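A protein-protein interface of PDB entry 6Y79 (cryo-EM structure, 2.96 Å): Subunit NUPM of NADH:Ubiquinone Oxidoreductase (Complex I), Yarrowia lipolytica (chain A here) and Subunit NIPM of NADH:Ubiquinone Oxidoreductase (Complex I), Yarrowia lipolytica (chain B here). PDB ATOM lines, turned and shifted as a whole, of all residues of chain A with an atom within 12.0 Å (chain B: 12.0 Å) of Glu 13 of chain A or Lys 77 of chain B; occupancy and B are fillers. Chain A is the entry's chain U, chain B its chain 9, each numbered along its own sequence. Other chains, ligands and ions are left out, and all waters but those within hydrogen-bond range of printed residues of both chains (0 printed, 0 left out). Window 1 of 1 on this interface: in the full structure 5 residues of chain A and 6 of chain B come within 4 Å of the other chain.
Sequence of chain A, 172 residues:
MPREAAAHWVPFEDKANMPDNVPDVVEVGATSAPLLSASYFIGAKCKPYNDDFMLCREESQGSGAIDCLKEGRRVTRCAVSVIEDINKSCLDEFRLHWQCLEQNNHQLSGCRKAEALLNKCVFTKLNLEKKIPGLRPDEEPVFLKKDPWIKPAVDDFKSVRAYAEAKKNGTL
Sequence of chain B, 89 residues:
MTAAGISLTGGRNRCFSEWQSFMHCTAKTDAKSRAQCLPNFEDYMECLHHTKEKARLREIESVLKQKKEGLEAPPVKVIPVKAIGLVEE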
ATOM      1  N   TRP A   9     -14.723 -23.655 -17.840  1.00  0.00           N
ATOM      2  CA  TRP A   9     -16.054 -24.067 -18.254  1.00  0.00           C
ATOM      3  C   TRP A   9     -16.808 -22.839 -18.754  1.00  0.00           C
ATOM      4  O   TRP A   9     -16.682 -21.748 -18.197  1.00  0.00           O
ATOM      5  CB  TRP A   9     -16.802 -24.708 -17.082  1.00  0.00           C
ATOM      6  CG  TRP A   9     -17.005 -23.776 -15.903  1.00  0.00           C
ATOM      7  CD1 TRP A   9     -16.121 -23.512 -14.898  1.00  0.00           C
ATOM      8  CD2 TRP A   9     -18.160 -22.975 -15.639  1.00  0.00           C
ATOM      9  NE1 TRP A   9     -16.659 -22.597 -14.024  1.00  0.00           N
ATOM     10  CE2 TRP A   9     -17.912 -22.254 -14.458  1.00  0.00           C
ATOM     11  CE3 TRP A   9     -19.379 -22.799 -16.289  1.00  0.00           C
ATOM     12  CZ2 TRP A   9     -18.842 -21.372 -13.915  1.00  0.00           C
ATOM     13  CZ3 TRP A   9     -20.302 -21.935 -15.743  1.00  0.00           C
ATOM     14  CH2 TRP A   9     -20.028 -21.226 -14.573  1.00  0.00           C
ATOM     15  N   VAL A  10     -17.589 -23.004 -19.818  1.00  0.00           N
ATOM     16  CA  VAL A  10     -18.484 -21.946 -20.274  1.00  0.00           C
ATOM     17  C   VAL A  10     -19.922 -22.440 -20.245  1.00  0.00           C
ATOM     18  O   VAL A  10     -20.206 -23.569 -20.658  1.00  0.00           O
ATOM     19  CB  VAL A  10     -18.114 -21.345 -21.649  1.00  0.00           C
ATOM     20  CG1 VAL A  10     -16.712 -20.752 -21.586  1.00  0.00           C
ATOM     21  CG2 VAL A  10     -18.251 -22.329 -22.848  1.00  0.00           C
ATOM     22  N   PRO A  11     -20.850 -21.667 -19.683  1.00  0.00           N
ATOM     23  CA  PRO A  11     -22.216 -22.157 -19.492  1.00  0.00           C
ATOM     24  C   PRO A  11     -23.056 -22.027 -20.749  1.00  0.00           C
ATOM     25  O   PRO A  11     -22.860 -21.129 -21.570  1.00  0.00           O
ATOM     26  CB  PRO A  11     -22.755 -21.270 -18.364  1.00  0.00           C
ATOM     27  CG  PRO A  11     -21.919 -20.062 -18.384  1.00  0.00           C
ATOM     28  CD  PRO A  11     -20.599 -20.401 -18.970  1.00  0.00           C
ATOM     29  N   PHE A  12     -23.999 -22.945 -20.900  1.00  0.00           N
ATOM     30  CA  PHE A  12     -24.834 -22.940 -22.087  1.00  0.00           C
ATOM     31  C   PHE A  12     -26.222 -23.453 -21.753  1.00  0.00           C
ATOM     32  O   PHE A  12     -26.384 -24.340 -20.910  1.00  0.00           O
ATOM     33  CB  PHE A  12     -24.222 -23.764 -23.239  1.00  0.00           C
ATOM     34  CG  PHE A  12     -24.181 -25.237 -22.993  1.00  0.00           C
ATOM     35  CD1 PHE A  12     -23.186 -25.788 -22.214  1.00  0.00           C
ATOM     36  CD2 PHE A  12     -25.118 -26.078 -23.569  1.00  0.00           C
ATOM     37  CE1 PHE A  12     -23.140 -27.139 -21.988  1.00  0.00           C
ATOM     38  CE2 PHE A  12     -25.072 -27.437 -23.345  1.00  0.00           C
ATOM     39  CZ  PHE A  12     -24.090 -27.963 -22.550  1.00  0.00           C
ATOM     40  N   GLU A  13     -27.218 -22.888 -22.417  1.00  0.00           N
ATOM     41  CA  GLU A  13     -28.591 -23.272 -22.176  1.00  0.00           C
ATOM     42  C   GLU A  13     -29.298 -23.604 -23.474  1.00  0.00           C
ATOM     43  O   GLU A  13     -28.761 -23.419 -24.565  1.00  0.00           O
ATOM     44  CB  GLU A  13     -29.347 -22.188 -21.426  1.00  0.00           C
ATOM     45  CG  GLU A  13     -29.639 -20.961 -22.158  1.00  0.00           C
ATOM     46  CD  GLU A  13     -28.571 -19.884 -22.018  1.00  0.00           C
ATOM     47  OE1 GLU A  13     -27.396 -20.184 -21.751  1.00  0.00           O
ATOM     48  OE2 GLU A  13     -28.984 -18.717 -22.035  1.00  0.00           O
ATOM     49  N   ASP A  14     -30.534 -24.067 -23.335  1.00  0.00           N
ATOM     50  CA  ASP A  14     -31.166 -24.836 -24.393  1.00  0.00           C
ATOM     51  C   ASP A  14     -32.569 -24.316 -24.672  1.00  0.00           C
ATOM     52  O   ASP A  14     -33.460 -24.401 -23.817  1.00  0.00           O
ATOM     53  CB  ASP A  14     -31.185 -26.311 -24.020  1.00  0.00           C
ATOM     54  CG  ASP A  14     -31.843 -27.149 -25.065  1.00  0.00           C
ATOM     55  OD1 ASP A  14     -31.277 -27.314 -26.166  1.00  0.00           O
ATOM     56  OD2 ASP A  14     -32.920 -27.677 -24.759  1.00  0.00           O
ATOM     57  N   LYS A  15     -32.752 -23.795 -25.881  1.00  0.00           N
ATOM     58  CA  LYS A  15     -34.046 -23.276 -26.303  1.00  0.00           C
ATOM     59  C   LYS A  15     -34.999 -24.387 -26.680  1.00  0.00           C
ATOM     60  O   LYS A  15     -35.282 -24.560 -27.863  1.00  0.00           O
ATOM     61  CB  LYS A  15     -33.904 -22.376 -27.519  1.00  0.00           C
ATOM     62  CG  LYS A  15     -33.588 -20.976 -27.272  1.00  0.00           C
ATOM     63  CD  LYS A  15     -32.111 -20.725 -27.385  1.00  0.00           C
ATOM     64  CE  LYS A  15     -31.949 -19.237 -27.613  1.00  0.00           C
ATOM     65  NZ  LYS A  15     -30.555 -18.755 -27.862  1.00  0.00           N
ATOM     66  N   ALA A  16     -35.574 -25.100 -25.716  1.00  0.00           N
ATOM     67  CA  ALA A  16     -36.444 -26.180 -26.145  1.00  0.00           C
ATOM     68  C   ALA A  16     -37.553 -26.417 -25.152  1.00  0.00           C
ATOM     69  O   ALA A  16     -37.726 -25.679 -24.185  1.00  0.00           O
ATOM     70  CB  ALA A  16     -35.674 -27.459 -26.382  1.00  0.00           C
ATOM     71  N   ASN A  17     -38.292 -27.480 -25.406  1.00  0.00           N
ATOM     72  CA  ASN A  17     -39.491 -27.794 -24.660  1.00  0.00           C
ATOM     73  C   ASN A  17     -39.526 -29.277 -24.328  1.00  0.00           C
ATOM     74  O   ASN A  17     -38.882 -30.094 -24.997  1.00  0.00           O
ATOM     75  CB  ASN A  17     -40.750 -27.420 -25.458  1.00  0.00           C
ATOM     76  CG  ASN A  17     -40.928 -25.923 -25.607  1.00  0.00           C
ATOM     77  OD1 ASN A  17     -40.730 -25.169 -24.659  1.00  0.00           O
ATOM     78  ND2 ASN A  17     -41.300 -25.487 -26.801  1.00  0.00           N
ATOM     79  N   LEU B  71     -27.348 -24.829 -39.145  1.00  0.00           N
ATOM     80  CA  LEU B  71     -28.219 -25.288 -38.066  1.00  0.00           C
ATOM     81  C   LEU B  71     -29.598 -24.671 -38.244  1.00  0.00           C
ATOM     82  O   LEU B  71     -29.738 -23.445 -38.250  1.00  0.00           O
ATOM     83  CB  LEU B  71     -27.619 -24.944 -36.698  1.00  0.00           C
ATOM     84  CG  LEU B  71     -28.247 -25.425 -35.388  1.00  0.00           C
ATOM     85  CD1 LEU B  71     -27.143 -25.818 -34.421  1.00  0.00           C
ATOM     86  CD2 LEU B  71     -29.120 -24.342 -34.753  1.00  0.00           C
ATOM     87  N   ALA B  73     -32.738 -25.471 -36.229  1.00  0.00           N
ATOM     88  CA  ALA B  73     -32.963 -26.231 -35.020  1.00  0.00           C
ATOM     89  C   ALA B  73     -33.333 -25.247 -33.926  1.00  0.00           C
ATOM     90  O   ALA B  73     -33.161 -24.026 -34.080  1.00  0.00           O
ATOM     91  CB  ALA B  73     -31.710 -27.008 -34.616  1.00  0.00           C
ATOM     92  N   PRO B  74     -33.874 -25.732 -32.820  1.00  0.00           N
ATOM     93  CA  PRO B  74     -33.784 -24.996 -31.575  1.00  0.00           C
ATOM     94  C   PRO B  74     -32.335 -24.892 -31.136  1.00  0.00           C
ATOM     95  O   PRO B  74     -31.728 -25.895 -30.732  1.00  0.00           O
ATOM     96  CB  PRO B  74     -34.603 -25.864 -30.617  1.00  0.00           C
ATOM     97  CG  PRO B  74     -35.625 -26.473 -31.478  1.00  0.00           C
ATOM     98  CD  PRO B  74     -34.910 -26.778 -32.759  1.00  0.00           C
ATOM     99  N   PRO B  75     -31.746 -23.702 -31.191  1.00  0.00           N
ATOM    100  CA  PRO B  75     -30.302 -23.578 -30.976  1.00  0.00           C
ATOM    101  C   PRO B  75     -29.962 -23.596 -29.490  1.00  0.00           C
ATOM    102  O   PRO B  75     -30.834 -23.671 -28.626  1.00  0.00           O
ATOM    103  CB  PRO B  75     -29.977 -22.224 -31.608  1.00  0.00           C
ATOM    104  CG  PRO B  75     -31.215 -21.413 -31.341  1.00  0.00           C
ATOM    105  CD  PRO B  75     -32.388 -22.384 -31.331  1.00  0.00           C
ATOM    106  N   VAL B  76     -28.663 -23.548 -29.199  1.00  0.00           N
ATOM    107  CA  VAL B  76     -28.184 -23.434 -27.827  1.00  0.00           C
ATOM    108  C   VAL B  76     -27.446 -22.110 -27.664  1.00  0.00           C
ATOM    109  O   VAL B  76     -26.686 -21.678 -28.546  1.00  0.00           O
ATOM    110  CB  VAL B  76     -27.322 -24.635 -27.399  1.00  0.00           C
ATOM    111  CG1 VAL B  76     -28.170 -25.890 -27.360  1.00  0.00           C
ATOM    112  CG2 VAL B  76     -26.105 -24.847 -28.291  1.00  0.00           C
ATOM    113  N   LYS B  77     -27.726 -21.448 -26.544  1.00  0.00           N
ATOM    114  CA  LYS B  77     -27.196 -20.132 -26.207  1.00  0.00           C
ATOM    115  C   LYS B  77     -25.966 -20.304 -25.347  1.00  0.00           C
ATOM    116  O   LYS B  77     -25.879 -21.269 -24.608  1.00  0.00           O
ATOM    117  CB  LYS B  77     -28.237 -19.335 -25.459  1.00  0.00           C
ATOM    118  CG  LYS B  77     -27.880 -17.962 -24.909  1.00  0.00           C
ATOM    119  CD  LYS B  77     -28.056 -16.862 -25.957  1.00  0.00           C
ATOM    120  CE  LYS B  77     -28.056 -15.533 -25.277  1.00  0.00           C
ATOM    121  NZ  LYS B  77     -26.798 -15.470 -24.516  1.00  0.00           N
ATOM    122  N   VAL B  78     -25.003 -19.426 -25.486  1.00  0.00           N
ATOM    123  CA  VAL B  78     -23.929 -19.316 -24.500  1.00  0.00           C
ATOM    124  C   VAL B  78     -24.084 -18.006 -23.741  1.00  0.00           C
ATOM    125  O   VAL B  78     -24.407 -16.971 -24.331  1.00  0.00           O
ATOM    126  CB  VAL B  78     -22.558 -19.436 -25.187  1.00  0.00           C
ATOM    127  CG1 VAL B  78     -21.405 -19.010 -24.289  1.00  0.00           C
ATOM    128  CG2 VAL B  78     -22.399 -20.853 -25.581  1.00  0.00           C
ATOM    129  N   ILE B  79     -23.919 -18.062 -22.423  1.00  0.00           N
ATOM    130  CA  ILE B  79     -24.003 -16.875 -21.581  1.00  0.00           C
ATOM    131  C   ILE B  79     -22.646 -16.564 -20.966  1.00  0.00           C
ATOM    132  O   ILE B  79     -21.785 -17.452 -20.884  1.00  0.00           O
ATOM    133  CB  ILE B  79     -25.056 -17.072 -20.485  1.00  0.00           C
ATOM    134  CG1 ILE B  79     -24.861 -18.438 -19.838  1.00  0.00           C
ATOM    135  CG2 ILE B  79     -26.448 -16.901 -21.047  1.00  0.00           C
ATOM    136  CD1 ILE B  79     -25.721 -18.697 -18.683  1.00  0.00           C
ATOM    137  N   PRO B  80     -22.404 -15.327 -20.549  1.00  0.00           N
ATOM    138  CA  PRO B  80     -21.362 -15.088 -19.553  1.00  0.00           C
ATOM    139  C   PRO B  80     -21.836 -15.558 -18.189  1.00  0.00           C
ATOM    140  O   PRO B  80     -23.033 -15.673 -17.919  1.00  0.00           O
ATOM    141  CB  PRO B  80     -21.174 -13.569 -19.581  1.00  0.00           C
ATOM    142  CG  PRO B  80     -22.486 -13.047 -20.058  1.00  0.00           C
ATOM    143  CD  PRO B  80     -23.003 -14.069 -21.037  1.00  0.00           C
ATOM    144  N   VAL B  81     -20.859 -15.792 -17.309  1.00  0.00           N
ATOM    145  CA  VAL B  81     -21.142 -16.251 -15.949  1.00  0.00           C
ATOM    146  C   VAL B  81     -21.823 -15.158 -15.125  1.00  0.00           C
ATOM    147  O   VAL B  81     -22.392 -15.430 -14.062  1.00  0.00           O
ATOM    148  CB  VAL B  81     -19.837 -16.747 -15.297  1.00  0.00           C
ATOM    149  CG1 VAL B  81     -19.119 -17.703 -16.237  1.00  0.00           C
ATOM    150  CG2 VAL B  81     -18.936 -15.582 -14.950  1.00  0.00           C
ATOM    151  N   LYS B  82     -21.796 -13.921 -15.611  1.00  0.00           N
ATOM    152  CA  LYS B  82     -22.456 -12.780 -15.002  1.00  0.00           C
ATOM    153  C   LYS B  82     -23.971 -12.800 -15.207  1.00  0.00           C
ATOM    154  O   LYS B  82     -24.672 -11.986 -14.602  1.00  0.00           O
ATOM    155  CB  LYS B  82     -21.871 -11.499 -15.586  1.00  0.00           C
ATOM    156  CG  LYS B  82     -20.351 -11.475 -15.638  1.00  0.00           C
ATOM    157  CD  LYS B  82     -19.842 -11.052 -17.022  1.00  0.00           C
ATOM    158  CE  LYS B  82     -18.375 -11.452 -17.177  1.00  0.00           C
ATOM    159  NZ  LYS B  82     -17.924 -11.719 -18.571  1.00  0.00           N
ATOM    160  N   ALA B  83     -24.487 -13.676 -16.070  1.00  0.00           N
ATOM    161  CA  ALA B  83     -25.829 -13.537 -16.635  1.00  0.00           C
ATOM    162  C   ALA B  83     -26.541 -14.884 -16.747  1.00  0.00           C
ATOM    163  O   ALA B  83     -27.081 -15.237 -17.799  1.00  0.00           O
ATOM    164  CB  ALA B  83     -25.742 -12.860 -17.990  1.00  0.00           C
ATOM    165  N   ILE B  84     -26.537 -15.679 -15.673  1.00  0.00           N
ATOM    166  CA  ILE B  84     -27.186 -16.993 -15.724  1.00  0.00           C
ATOM    167  C   ILE B  84     -28.708 -16.849 -15.639  1.00  0.00           C
ATOM    168  O   ILE B  84     -29.460 -17.511 -16.370  1.00  0.00           O
ATOM    169  CB  ILE B  84     -26.613 -17.920 -14.632  1.00  0.00           C
ATOM    170  CG1 ILE B  84     -25.163 -18.253 -14.991  1.00  0.00           C
ATOM    171  CG2 ILE B  84     -27.443 -19.195 -14.431  1.00  0.00           C
ATOM    172  CD1 ILE B  84     -24.495 -19.263 -14.102  1.00  0.00           C
ATOM    173  N   GLY B  85     -29.182 -15.945 -14.791  1.00  0.00           N
ATOM    174  CA  GLY B  85     -30.609 -15.744 -14.691  1.00  0.00           C
ATOM    175  C   GLY B  85     -31.067 -14.339 -15.021  1.00  0.00           C
ATOM    176  O   GLY B  85     -31.937 -13.817 -14.329  1.00  0.00           O
ATOM    177  N   LEU B  86     -30.521 -13.725 -16.077  1.00  0.00           N
ATOM    178  CA  LEU B  86     -30.656 -12.280 -16.271  1.00  0.00           C
ATOM    179  C   LEU B  86     -32.091 -11.869 -16.599  1.00  0.00           C
ATOM    180  O   LEU B  86     -32.726 -11.138 -15.833  1.00  0.00           O
ATOM    181  CB  LEU B  86     -29.696 -11.812 -17.369  1.00  0.00           C
ATOM    182  CG  LEU B  86     -29.604 -10.303 -17.593  1.00  0.00           C
ATOM    183  CD1 LEU B  86     -29.186  -9.588 -16.318  1.00  0.00           C
ATOM    184  CD2 LEU B  86     -28.615 -10.010 -18.706  1.00  0.00           C
ATOM    185  N   VAL B  87     -32.624 -12.335 -17.726  1.00  0.00           N
ATOM    186  CA  VAL B  87     -33.976 -11.946 -18.102  1.00  0.00           C
ATOM    187  C   VAL B  87     -34.991 -12.788 -17.342  1.00  0.00           C
ATOM    188  O   VAL B  87     -35.538 -12.351 -16.331  1.00  0.00           O
ATOM    189  CB  VAL B  87     -34.212 -12.061 -19.614  1.00  0.00           C
ATOM    190  CG1 VAL B  87     -33.925 -13.476 -20.095  1.00  0.00           C
ATOM    191  CG2 VAL B  87     -35.634 -11.656 -19.947  1.00  0.00           C
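The backbone carbonyl oxygen (O) of Pro 75 of chain B sits at hydrogen-bond distance from the backbone NH (N) of Lys 15 of chain A. The backbone carbonyl oxygen of Glu 13 of chain A is in hydrogen-bond range of the backbone NH of Lys 77 of chain B (3.0 Å). The backbone carbonyl oxygen (O) of Pro 11 of chain A lies within hydrogen-bond range of the backbone NH (N) of Ile 79 of chain B, at 3.4 Å.
Pro 11 of chain A touches Val 78 of chain B. Phe 12 of chain A touches Lys 77 of chain B. O of Glu 13 of chain A touches CA of Val 76 of chain B, at 3.3 Å. CG2 of Ile 79 of chain B touches OE2 of Glu 13 of chain A, 3.3 Å away. Asp 14 of chain A touches Val 76 of chain B. O of Lys 15 of chain A touches CB of Pro 74 of chain B (3.1 Å). CB of Lys 77 of chain B touches NZ of Lys 15 of chain A, at 3.4 Å.
Of chain B, only Lys 77 comes within 4 Å of Phe 12 of chain A. Glu 13 of chain A touches just these residues of chain B: Val 76, Lys 77 and Ile 79. Lys 15 of chain A touches just these residues of chain B: Pro 74 (3.1 Å), Pro 75 (3.4 Å) and Lys 77 (3.4 Å). Of the printed residues of chain A, Pro 74 of chain B touches Lys 15. Of the printed residues of chain A, Pro 75 of chain B touches Lys 15 (3.4 Å). Val 76 of chain B touches just these residues of chain A: Glu 13 (3.3 Å) and Asp 14 (3.6 Å). Lys 77 of chain B touches just these residues of chain A: Phe 12, Glu 13 and Lys 15. Gly 85 of chain B touches none of the printed residues of chain A. The nearest residue of chain B that does not touch Glu 13 of chain A is Val 78 of chain B (4.4 Å).
Of the 16 printed residues of chain B, 6 touch a printed residue of chain A. Printed residues of chain B that touch a printed residue of chain A: Pro 74, Pro 75, Val 76, Lys 77, Val 78 and Ile 79. Hydrophobic or aromatic side chains of chain B that line the printed part of chain A: Pro 74, Val 76, Val 78 and Ile 79. Hydrophobic or aromatic side chains of chain A within 4 Å of the printed part of chain B: Pro 11 and Phe 12. Among the printed residues, 10 pairs touch across the chains. Among the printed residues, no Asp or Glu carboxylate lies within 4 Å of a Lys or Arg side-chain nitrogen of the other chain.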
